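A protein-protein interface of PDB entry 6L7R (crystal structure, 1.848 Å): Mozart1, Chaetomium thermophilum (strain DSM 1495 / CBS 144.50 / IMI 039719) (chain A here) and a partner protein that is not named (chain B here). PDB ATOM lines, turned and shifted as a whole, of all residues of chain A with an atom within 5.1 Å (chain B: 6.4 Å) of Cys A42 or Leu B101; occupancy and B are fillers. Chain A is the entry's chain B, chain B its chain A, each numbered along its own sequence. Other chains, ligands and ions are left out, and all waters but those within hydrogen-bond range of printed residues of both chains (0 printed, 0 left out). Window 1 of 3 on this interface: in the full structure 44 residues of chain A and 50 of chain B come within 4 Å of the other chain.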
ATOM      1  N   LEU A  34      -9.277 -16.853   7.145  1.00  0.00           N
ATOM      2  CA  LEU A  34      -8.990 -17.786   8.228  1.00  0.00           C
ATOM      3  C   LEU A  34      -8.386 -19.060   7.650  1.00  0.00           C
ATOM      4  O   LEU A  34      -8.952 -19.645   6.721  1.00  0.00           O
ATOM      5  CB  LEU A  34     -10.258 -18.142   9.007  1.00  0.00           C
ATOM      6  CG  LEU A  34     -10.973 -17.131   9.895  1.00  0.00           C
ATOM      7  CD1 LEU A  34     -12.382 -17.634  10.155  1.00  0.00           C
ATOM      8  CD2 LEU A  34     -10.222 -16.958  11.215  1.00  0.00           C
ATOM      9  N   THR A  38      -6.649 -21.634  12.592  1.00  0.00           N
ATOM     10  CA  THR A  38      -7.347 -20.601  13.354  1.00  0.00           C
ATOM     11  C   THR A  38      -8.828 -20.926  13.466  1.00  0.00           C
ATOM     12  O   THR A  38      -9.439 -20.745  14.527  1.00  0.00           O
ATOM     13  CB  THR A  38      -7.133 -19.242  12.699  1.00  0.00           C
ATOM     14  OG1 THR A  38      -5.727 -19.043  12.503  1.00  0.00           O
ATOM     15  CG2 THR A  38      -7.696 -18.119  13.568  1.00  0.00           C
ATOM     16  N   LEU A  39      -9.414 -21.430  12.380  1.00  0.00           N
ATOM     17  CA  LEU A  39     -10.813 -21.830  12.421  1.00  0.00           C
ATOM     18  C   LEU A  39     -11.045 -22.875  13.502  1.00  0.00           C
ATOM     19  O   LEU A  39     -12.000 -22.781  14.279  1.00  0.00           O
ATOM     20  CB  LEU A  39     -11.232 -22.360  11.050  1.00  0.00           C
ATOM     21  CG  LEU A  39     -12.636 -22.940  10.948  1.00  0.00           C
ATOM     22  CD1 LEU A  39     -13.693 -21.917  11.316  1.00  0.00           C
ATOM     23  CD2 LEU A  39     -12.834 -23.430   9.511  1.00  0.00           C
ATOM     24  N   SER A  40     -10.183 -23.897  13.551  1.00  0.00           N
ATOM     25  CA  SER A  40     -10.362 -24.970  14.517  1.00  0.00           C
ATOM     26  C   SER A  40     -10.234 -24.453  15.937  1.00  0.00           C
ATOM     27  O   SER A  40     -10.976 -24.887  16.828  1.00  0.00           O
ATOM     28  CB  SER A  40      -9.352 -26.090  14.261  1.00  0.00           C
ATOM     29  OG  SER A  40      -9.657 -26.753  13.042  1.00  0.00           O
ATOM     30  N   ILE A  41      -9.310 -23.514  16.174  1.00  0.00           N
ATOM     31  CA  ILE A  41      -9.225 -22.913  17.505  1.00  0.00           C
ATOM     32  C   ILE A  41     -10.521 -22.193  17.842  1.00  0.00           C
ATOM     33  O   ILE A  41     -11.064 -22.335  18.944  1.00  0.00           O
ATOM     34  CB  ILE A  41      -8.019 -21.960  17.609  1.00  0.00           C
ATOM     35  CG1 ILE A  41      -6.702 -22.725  17.452  1.00  0.00           C
ATOM     36  CG2 ILE A  41      -8.063 -21.238  18.951  1.00  0.00           C
ATOM     37  CD1 ILE A  41      -5.496 -21.793  17.341  1.00  0.00           C
ATOM     38  N   CYS A  42     -11.029 -21.395  16.900  1.00  0.00           N
ATOM     39  CA  CYS A  42     -12.257 -20.649  17.149  1.00  0.00           C
ATOM     40  C   CYS A  42     -13.422 -21.591  17.420  1.00  0.00           C
ATOM     41  O   CYS A  42     -14.220 -21.361  18.342  1.00  0.00           O
ATOM     42  CB  CYS A  42     -12.569 -19.742  15.958  1.00  0.00           C
ATOM     43  SG  CYS A  42     -11.450 -18.304  15.816  1.00  0.00           S
ATOM     44  N   ILE A  43     -13.540 -22.650  16.618  1.00  0.00           N
ATOM     45  CA  ILE A  43     -14.591 -23.646  16.851  1.00  0.00           C
ATOM     46  C   ILE A  43     -14.512 -24.162  18.285  1.00  0.00           C
ATOM     47  O   ILE A  43     -15.519 -24.227  19.005  1.00  0.00           O
ATOM     48  CB  ILE A  43     -14.480 -24.787  15.821  1.00  0.00           C
ATOM     49  CG1 ILE A  43     -14.834 -24.288  14.424  1.00  0.00           C
ATOM     50  CG2 ILE A  43     -15.381 -25.965  16.202  1.00  0.00           C
ATOM     51  CD1 ILE A  43     -14.497 -25.280  13.309  1.00  0.00           C
ATOM     52  N   SER A  44     -13.300 -24.490  18.733  1.00  0.00           N
ATOM     53  CA  SER A  44     -13.115 -25.023  20.080  1.00  0.00           C
ATOM     54  C   SER A  44     -13.585 -24.029  21.143  1.00  0.00           C
ATOM     55  O   SER A  44     -14.300 -24.399  22.081  1.00  0.00           O
ATOM     56  CB  SER A  44     -11.645 -25.377  20.295  1.00  0.00           C
ATOM     57  OG  SER A  44     -11.419 -25.729  21.642  1.00  0.00           O
ATOM     58  N   MET A  45     -13.182 -22.760  21.012  1.00  0.00           N
ATOM     59  CA  MET A  45     -13.601 -21.741  21.972  1.00  0.00           C
ATOM     60  C   MET A  45     -15.108 -21.527  21.937  1.00  0.00           C
ATOM     61  O   MET A  45     -15.746 -21.353  22.981  1.00  0.00           O
ATOM     62  CB  MET A  45     -12.859 -20.420  21.692  1.00  0.00           C
ATOM     63  CG  MET A  45     -11.373 -20.502  21.965  1.00  0.00           C
ATOM     64  SD  MET A  45     -10.344 -19.132  21.268  1.00  0.00           S
ATOM     65  CE  MET A  45     -10.878 -17.928  22.440  1.00  0.00           C
ATOM     66  N   ILE A  46     -15.700 -21.531  20.743  1.00  0.00           N
ATOM     67  CA  ILE A  46     -17.127 -21.273  20.667  1.00  0.00           C
ATOM     68  C   ILE A  46     -17.896 -22.433  21.270  1.00  0.00           C
ATOM     69  O   ILE A  46     -18.885 -22.234  21.989  1.00  0.00           O
ATOM     70  CB  ILE A  46     -17.534 -20.993  19.212  1.00  0.00           C
ATOM     71  CG1 ILE A  46     -17.138 -19.558  18.852  1.00  0.00           C
ATOM     72  CG2 ILE A  46     -19.042 -21.197  19.024  1.00  0.00           C
ATOM     73  CD1 ILE A  46     -17.422 -19.218  17.422  1.00  0.00           C
ATOM     74  N   GLU A  47     -17.425 -23.660  21.028  1.00  0.00           N
ATOM     75  CA  GLU A  47     -18.077 -24.839  21.597  1.00  0.00           C
ATOM     76  C   GLU A  47     -17.902 -24.900  23.112  1.00  0.00           C
ATOM     77  O   GLU A  47     -18.676 -25.587  23.793  1.00  0.00           O
ATOM     78  CB  GLU A  47     -17.533 -26.105  20.934  1.00  0.00           C
ATOM     79  CG  GLU A  47     -18.023 -26.282  19.491  1.00  0.00           C
ATOM     80  CD  GLU A  47     -19.548 -26.433  19.421  1.00  0.00           C
ATOM     81  OE1 GLU A  47     -20.089 -27.259  20.185  1.00  0.00           O
ATOM     82  OE2 GLU A  47     -20.207 -25.722  18.618  1.00  0.00           O
ATOM     83  N   PRO A  52     -19.440 -15.285  20.405  1.00  0.00           N
ATOM     84  CA  PRO A  52     -18.821 -15.219  19.076  1.00  0.00           C
ATOM     85  C   PRO A  52     -18.557 -13.808  18.600  1.00  0.00           C
ATOM     86  O   PRO A  52     -17.617 -13.594  17.828  1.00  0.00           O
ATOM     87  CB  PRO A  52     -19.850 -15.921  18.181  1.00  0.00           C
ATOM     88  CG  PRO A  52     -21.155 -15.623  18.858  1.00  0.00           C
ATOM     89  CD  PRO A  52     -20.847 -15.733  20.330  1.00  0.00           C
ATOM     90  N   LEU A  55     -15.325 -13.047  20.207  1.00  0.00           N
ATOM     91  CA  LEU A  55     -14.224 -13.777  19.580  1.00  0.00           C
ATOM     92  C   LEU A  55     -13.843 -13.147  18.242  1.00  0.00           C
ATOM     93  O   LEU A  55     -12.659 -13.101  17.877  1.00  0.00           O
ATOM     94  CB  LEU A  55     -14.596 -15.256  19.398  1.00  0.00           C
ATOM     95  CG  LEU A  55     -13.542 -16.152  18.729  1.00  0.00           C
ATOM     96  CD1 LEU A  55     -12.194 -16.005  19.421  1.00  0.00           C
ATOM     97  CD2 LEU A  55     -13.971 -17.604  18.774  1.00  0.00           C
ATOM     98  N   ALA A  56     -14.833 -12.654  17.493  1.00  0.00           N
ATOM     99  CA  ALA A  56     -14.521 -11.969  16.243  1.00  0.00           C
ATOM    100  C   ALA A  56     -13.684 -10.718  16.501  1.00  0.00           C
ATOM    101  O   ALA A  56     -12.741 -10.424  15.753  1.00  0.00           O
ATOM    102  CB  ALA A  56     -15.807 -11.617  15.502  1.00  0.00           C
ATOM    103  N   ILE A  59     -10.118 -11.871  17.153  1.00  0.00           N
ATOM    104  CA  ILE A  59      -9.377 -12.168  15.933  1.00  0.00           C
ATOM    105  C   ILE A  59      -8.948 -10.880  15.246  1.00  0.00           C
ATOM    106  O   ILE A  59      -7.813 -10.761  14.769  1.00  0.00           O
ATOM    107  CB  ILE A  59     -10.218 -13.049  14.983  1.00  0.00           C
ATOM    108  CG1 ILE A  59     -10.457 -14.422  15.597  1.00  0.00           C
ATOM    109  CG2 ILE A  59      -9.490 -13.194  13.646  1.00  0.00           C
ATOM    110  CD1 ILE A  59      -9.185 -15.235  15.798  1.00  0.00           C
ATOM    111  N   LEU B  16      -3.762 -19.277  19.833  1.00  0.00           N
ATOM    112  CA  LEU B  16      -4.095 -18.168  18.946  1.00  0.00           C
ATOM    113  C   LEU B  16      -3.011 -17.103  18.972  1.00  0.00           C
ATOM    114  O   LEU B  16      -2.577 -16.611  17.928  1.00  0.00           O
ATOM    115  CB  LEU B  16      -5.425 -17.535  19.360  1.00  0.00           C
ATOM    116  CG  LEU B  16      -6.782 -17.790  18.708  1.00  0.00           C
ATOM    117  CD1 LEU B  16      -7.711 -16.647  19.129  1.00  0.00           C
ATOM    118  CD2 LEU B  16      -6.709 -17.920  17.182  1.00  0.00           C
ATOM    119  N   ALA B  60     -27.677 -15.880  11.541  1.00  0.00           N
ATOM    120  CA  ALA B  60     -26.365 -15.686  10.932  1.00  0.00           C
ATOM    121  C   ALA B  60     -26.366 -16.111   9.470  1.00  0.00           C
ATOM    122  O   ALA B  60     -25.748 -15.455   8.624  1.00  0.00           O
ATOM    123  CB  ALA B  60     -25.300 -16.461  11.705  1.00  0.00           C
ATOM    124  N   TRP B  96     -24.927 -21.860  15.215  1.00  0.00           N
ATOM    125  CA  TRP B  96     -25.311 -20.470  14.976  1.00  0.00           C
ATOM    126  C   TRP B  96     -24.160 -19.522  15.291  1.00  0.00           C
ATOM    127  O   TRP B  96     -23.929 -18.543  14.574  1.00  0.00           O
ATOM    128  CB  TRP B  96     -26.534 -20.103  15.822  1.00  0.00           C
ATOM    129  CG  TRP B  96     -26.176 -19.851  17.268  1.00  0.00           C
ATOM    130  CD1 TRP B  96     -26.152 -20.767  18.282  1.00  0.00           C
ATOM    131  CD2 TRP B  96     -25.747 -18.603  17.845  1.00  0.00           C
ATOM    132  NE1 TRP B  96     -25.751 -20.166  19.453  1.00  0.00           N
ATOM    133  CE2 TRP B  96     -25.493 -18.841  19.212  1.00  0.00           C
ATOM    134  CE3 TRP B  96     -25.549 -17.315  17.335  1.00  0.00           C
ATOM    135  CZ2 TRP B  96     -25.059 -17.833  20.081  1.00  0.00           C
ATOM    136  CZ3 TRP B  96     -25.119 -16.312  18.199  1.00  0.00           C
ATOM    137  CH2 TRP B  96     -24.878 -16.580  19.555  1.00  0.00           C
ATOM    138  N   ALA B  97     -23.420 -19.801  16.356  1.00  0.00           N
ATOM    139  CA  ALA B  97     -22.405 -18.842  16.767  1.00  0.00           C
ATOM    140  C   ALA B  97     -21.166 -18.940  15.894  1.00  0.00           C
ATOM    141  O   ALA B  97     -20.500 -17.925  15.652  1.00  0.00           O
ATOM    142  CB  ALA B  97     -22.057 -19.049  18.243  1.00  0.00           C
ATOM    143  N   ILE B  98     -20.833 -20.142  15.413  1.00  0.00           N
ATOM    144  CA  ILE B  98     -19.701 -20.245  14.503  1.00  0.00           C
ATOM    145  C   ILE B  98     -20.000 -19.494  13.210  1.00  0.00           C
ATOM    146  O   ILE B  98     -19.147 -18.767  12.686  1.00  0.00           O
ATOM    147  CB  ILE B  98     -19.333 -21.716  14.255  1.00  0.00           C
ATOM    148  CG1 ILE B  98     -19.183 -22.434  15.605  1.00  0.00           C
ATOM    149  CG2 ILE B  98     -18.043 -21.778  13.464  1.00  0.00           C
ATOM    150  CD1 ILE B  98     -19.215 -23.957  15.560  1.00  0.00           C
ATOM    151  N   LEU B  99     -21.225 -19.614  12.704  1.00  0.00           N
ATOM    152  CA  LEU B  99     -21.591 -18.869  11.505  1.00  0.00           C
ATOM    153  C   LEU B  99     -21.617 -17.371  11.777  1.00  0.00           C
ATOM    154  O   LEU B  99     -21.254 -16.569  10.906  1.00  0.00           O
ATOM    155  CB  LEU B  99     -22.939 -19.350  10.972  1.00  0.00           C
ATOM    156  CG  LEU B  99     -22.903 -20.716  10.291  1.00  0.00           C
ATOM    157  CD1 LEU B  99     -24.303 -21.107   9.927  1.00  0.00           C
ATOM    158  CD2 LEU B  99     -22.036 -20.668   9.035  1.00  0.00           C
ATOM    159  N   TYR B 100     -22.052 -16.973  12.974  1.00  0.00           N
ATOM    160  CA  TYR B 100     -21.983 -15.562  13.336  1.00  0.00           C
ATOM    161  C   TYR B 100     -20.544 -15.064  13.297  1.00  0.00           C
ATOM    162  O   TYR B 100     -20.265 -13.978  12.772  1.00  0.00           O
ATOM    163  CB  TYR B 100     -22.587 -15.336  14.720  1.00  0.00           C
ATOM    164  CG  TYR B 100     -22.868 -13.877  14.995  1.00  0.00           C
ATOM    165  CD1 TYR B 100     -24.012 -13.270  14.495  1.00  0.00           C
ATOM    166  CD2 TYR B 100     -21.987 -13.101  15.738  1.00  0.00           C
ATOM    167  CE1 TYR B 100     -24.276 -11.946  14.724  1.00  0.00           C
ATOM    168  CE2 TYR B 100     -22.250 -11.762  15.972  1.00  0.00           C
ATOM    169  CZ  TYR B 100     -23.398 -11.194  15.467  1.00  0.00           C
ATOM    170  OH  TYR B 100     -23.681  -9.865  15.689  1.00  0.00           O
ATOM    171  N   LEU B 101     -19.615 -15.865  13.825  1.00  0.00           N
ATOM    172  CA  LEU B 101     -18.203 -15.499  13.783  1.00  0.00           C
ATOM    173  C   LEU B 101     -17.741 -15.277  12.351  1.00  0.00           C
ATOM    174  O   LEU B 101     -17.117 -14.259  12.039  1.00  0.00           O
ATOM    175  CB  LEU B 101     -17.354 -16.581  14.454  1.00  0.00           C
ATOM    176  CG  LEU B 101     -15.855 -16.421  14.188  1.00  0.00           C
ATOM    177  CD1 LEU B 101     -15.310 -15.243  14.992  1.00  0.00           C
ATOM    178  CD2 LEU B 101     -15.084 -17.694  14.483  1.00  0.00           C
ATOM    179  N   LEU B 102     -18.040 -16.228  11.458  1.00  0.00           N
ATOM    180  CA  LEU B 102     -17.639 -16.063  10.064  1.00  0.00           C
ATOM    181  C   LEU B 102     -18.240 -14.801   9.452  1.00  0.00           C
ATOM    182  O   LEU B 102     -17.543 -14.045   8.762  1.00  0.00           O
ATOM    183  CB  LEU B 102     -18.031 -17.298   9.250  1.00  0.00           C
ATOM    184  CG  LEU B 102     -17.384 -18.608   9.702  1.00  0.00           C
ATOM    185  CD1 LEU B 102     -17.694 -19.735   8.721  1.00  0.00           C
ATOM    186  CD2 LEU B 102     -15.885 -18.456   9.839  1.00  0.00           C
ATOM    187  N   HIS B 103     -19.529 -14.545   9.697  1.00  0.00           N
ATOM    188  CA  HIS B 103     -20.138 -13.330   9.159  1.00  0.00           C
ATOM    189  C   HIS B 103     -19.392 -12.086   9.629  1.00  0.00           C
ATOM    190  O   HIS B 103     -19.181 -11.146   8.850  1.00  0.00           O
ATOM    191  CB  HIS B 103     -21.605 -13.245   9.566  1.00  0.00           C
ATOM    192  CG  HIS B 103     -22.202 -11.885   9.372  1.00  0.00           C
ATOM    193  ND1 HIS B 103     -22.593 -11.409   8.138  1.00  0.00           N
ATOM    194  CD2 HIS B 103     -22.460 -10.892  10.256  1.00  0.00           C
ATOM    195  CE1 HIS B 103     -23.076 -10.186   8.271  1.00  0.00           C
ATOM    196  NE2 HIS B 103     -23.005  -9.849   9.548  1.00  0.00           N
ATOM    197  N   GLN B 104     -18.976 -12.065  10.897  1.00  0.00           N
ATOM    198  CA  GLN B 104     -18.274 -10.891  11.417  1.00  0.00           C
ATOM    199  C   GLN B 104     -16.917 -10.701  10.746  1.00  0.00           C
ATOM    200  O   GLN B 104     -16.477  -9.566  10.537  1.00  0.00           O
ATOM    201  CB  GLN B 104     -18.101 -11.017  12.933  1.00  0.00           C
ATOM    202  CG  GLN B 104     -19.404 -10.996  13.699  1.00  0.00           C
ATOM    203  CD  GLN B 104     -20.036  -9.617  13.738  1.00  0.00           C
ATOM    204  OE1 GLN B 104     -20.927  -9.301  12.945  1.00  0.00           O
ATOM    205  NE2 GLN B 104     -19.571  -8.785  14.663  1.00  0.00           N
ATOM    206  N   LEU B 105     -16.227 -11.795  10.436  1.00  0.00           N
ATOM    207  CA  LEU B 105     -14.929 -11.741   9.775  1.00  0.00           C
ATOM    208  C   LEU B 105     -15.030 -11.644   8.260  1.00  0.00           C
ATOM    209  O   LEU B 105     -13.992 -11.530   7.596  1.00  0.00           O
ATOM    210  CB  LEU B 105     -14.096 -12.969  10.161  1.00  0.00           C
ATOM    211  CG  LEU B 105     -13.808 -13.068  11.662  1.00  0.00           C
ATOM    212  CD1 LEU B 105     -13.149 -14.390  12.015  1.00  0.00           C
ATOM    213  CD2 LEU B 105     -12.951 -11.895  12.103  1.00  0.00           C
ATOM    214  N   ALA B 106     -16.235 -11.669   7.700  1.00  0.00           N
ATOM    215  CA  ALA B 106     -16.377 -11.646   6.248  1.00  0.00           C
ATOM    216  C   ALA B 106     -15.845 -10.335   5.689  1.00  0.00           C
ATOM    217  O   ALA B 106     -16.026  -9.272   6.287  1.00  0.00           O
ATOM    218  CB  ALA B 106     -17.841 -11.833   5.848  1.00  0.00           C
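Cys A42 touches just one residue of chain B: Leu B101. Of the printed residues of chain A, Leu B101 touches Cys A42 (3.6 Å), Ile A46 (3.97 Å) and Ala A56 (3.6 Å). Printed residues of chain A within 4 Å of Ile B98: Ile A46 (3.6 Å) and Glu A47 (3.7 Å). Of the printed residues of chain B, Ile A59 touches Leu B16. The nearest residue of chain B that does not touch Cys A42 is Leu B16 (4.9 Å). The nearest printed residue of chain A that does not touch Leu B101 is Pro A52 (4.01 Å). The nearest printed residue of chain A that does not touch Gln B104 is Pro A52 (5.2 Å).
Along chain A the printed residues that touch a printed residue of chain B span positions 34 to 59. Among the printed residues, no Asp or Glu carboxylate lies within 4 Å of a Lys or Arg side-chain nitrogen of the other chain.
CD1 of Leu A34 touches CD2 of Leu B102, at 3.6 Å. Leu A34 touches Leu B105. Cys A42 touches Leu B101. Ile A46 touches Ala B97. CB of Leu B101 touches CD1 of Ile A46 (3.97 Å). Trp B96 touches Pro A52 (CH2 to CG, 3.9 Å). O of Ala B97 touches CB of Pro A52, at 3.3 Å. Leu B101 touches Ala A56 (CD1 to CA, 3.6 Å). Gln B104 touches Ala A56 (CB to CB, 3.5 Å). O of Ala A56 touches CD2 of Leu B105, at 3.9 Å.
The backbone carbonyl oxygen (O) of Thr A38 lies within hydrogen-bond range of the side-chain sulfur (SG) of Cys A42.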
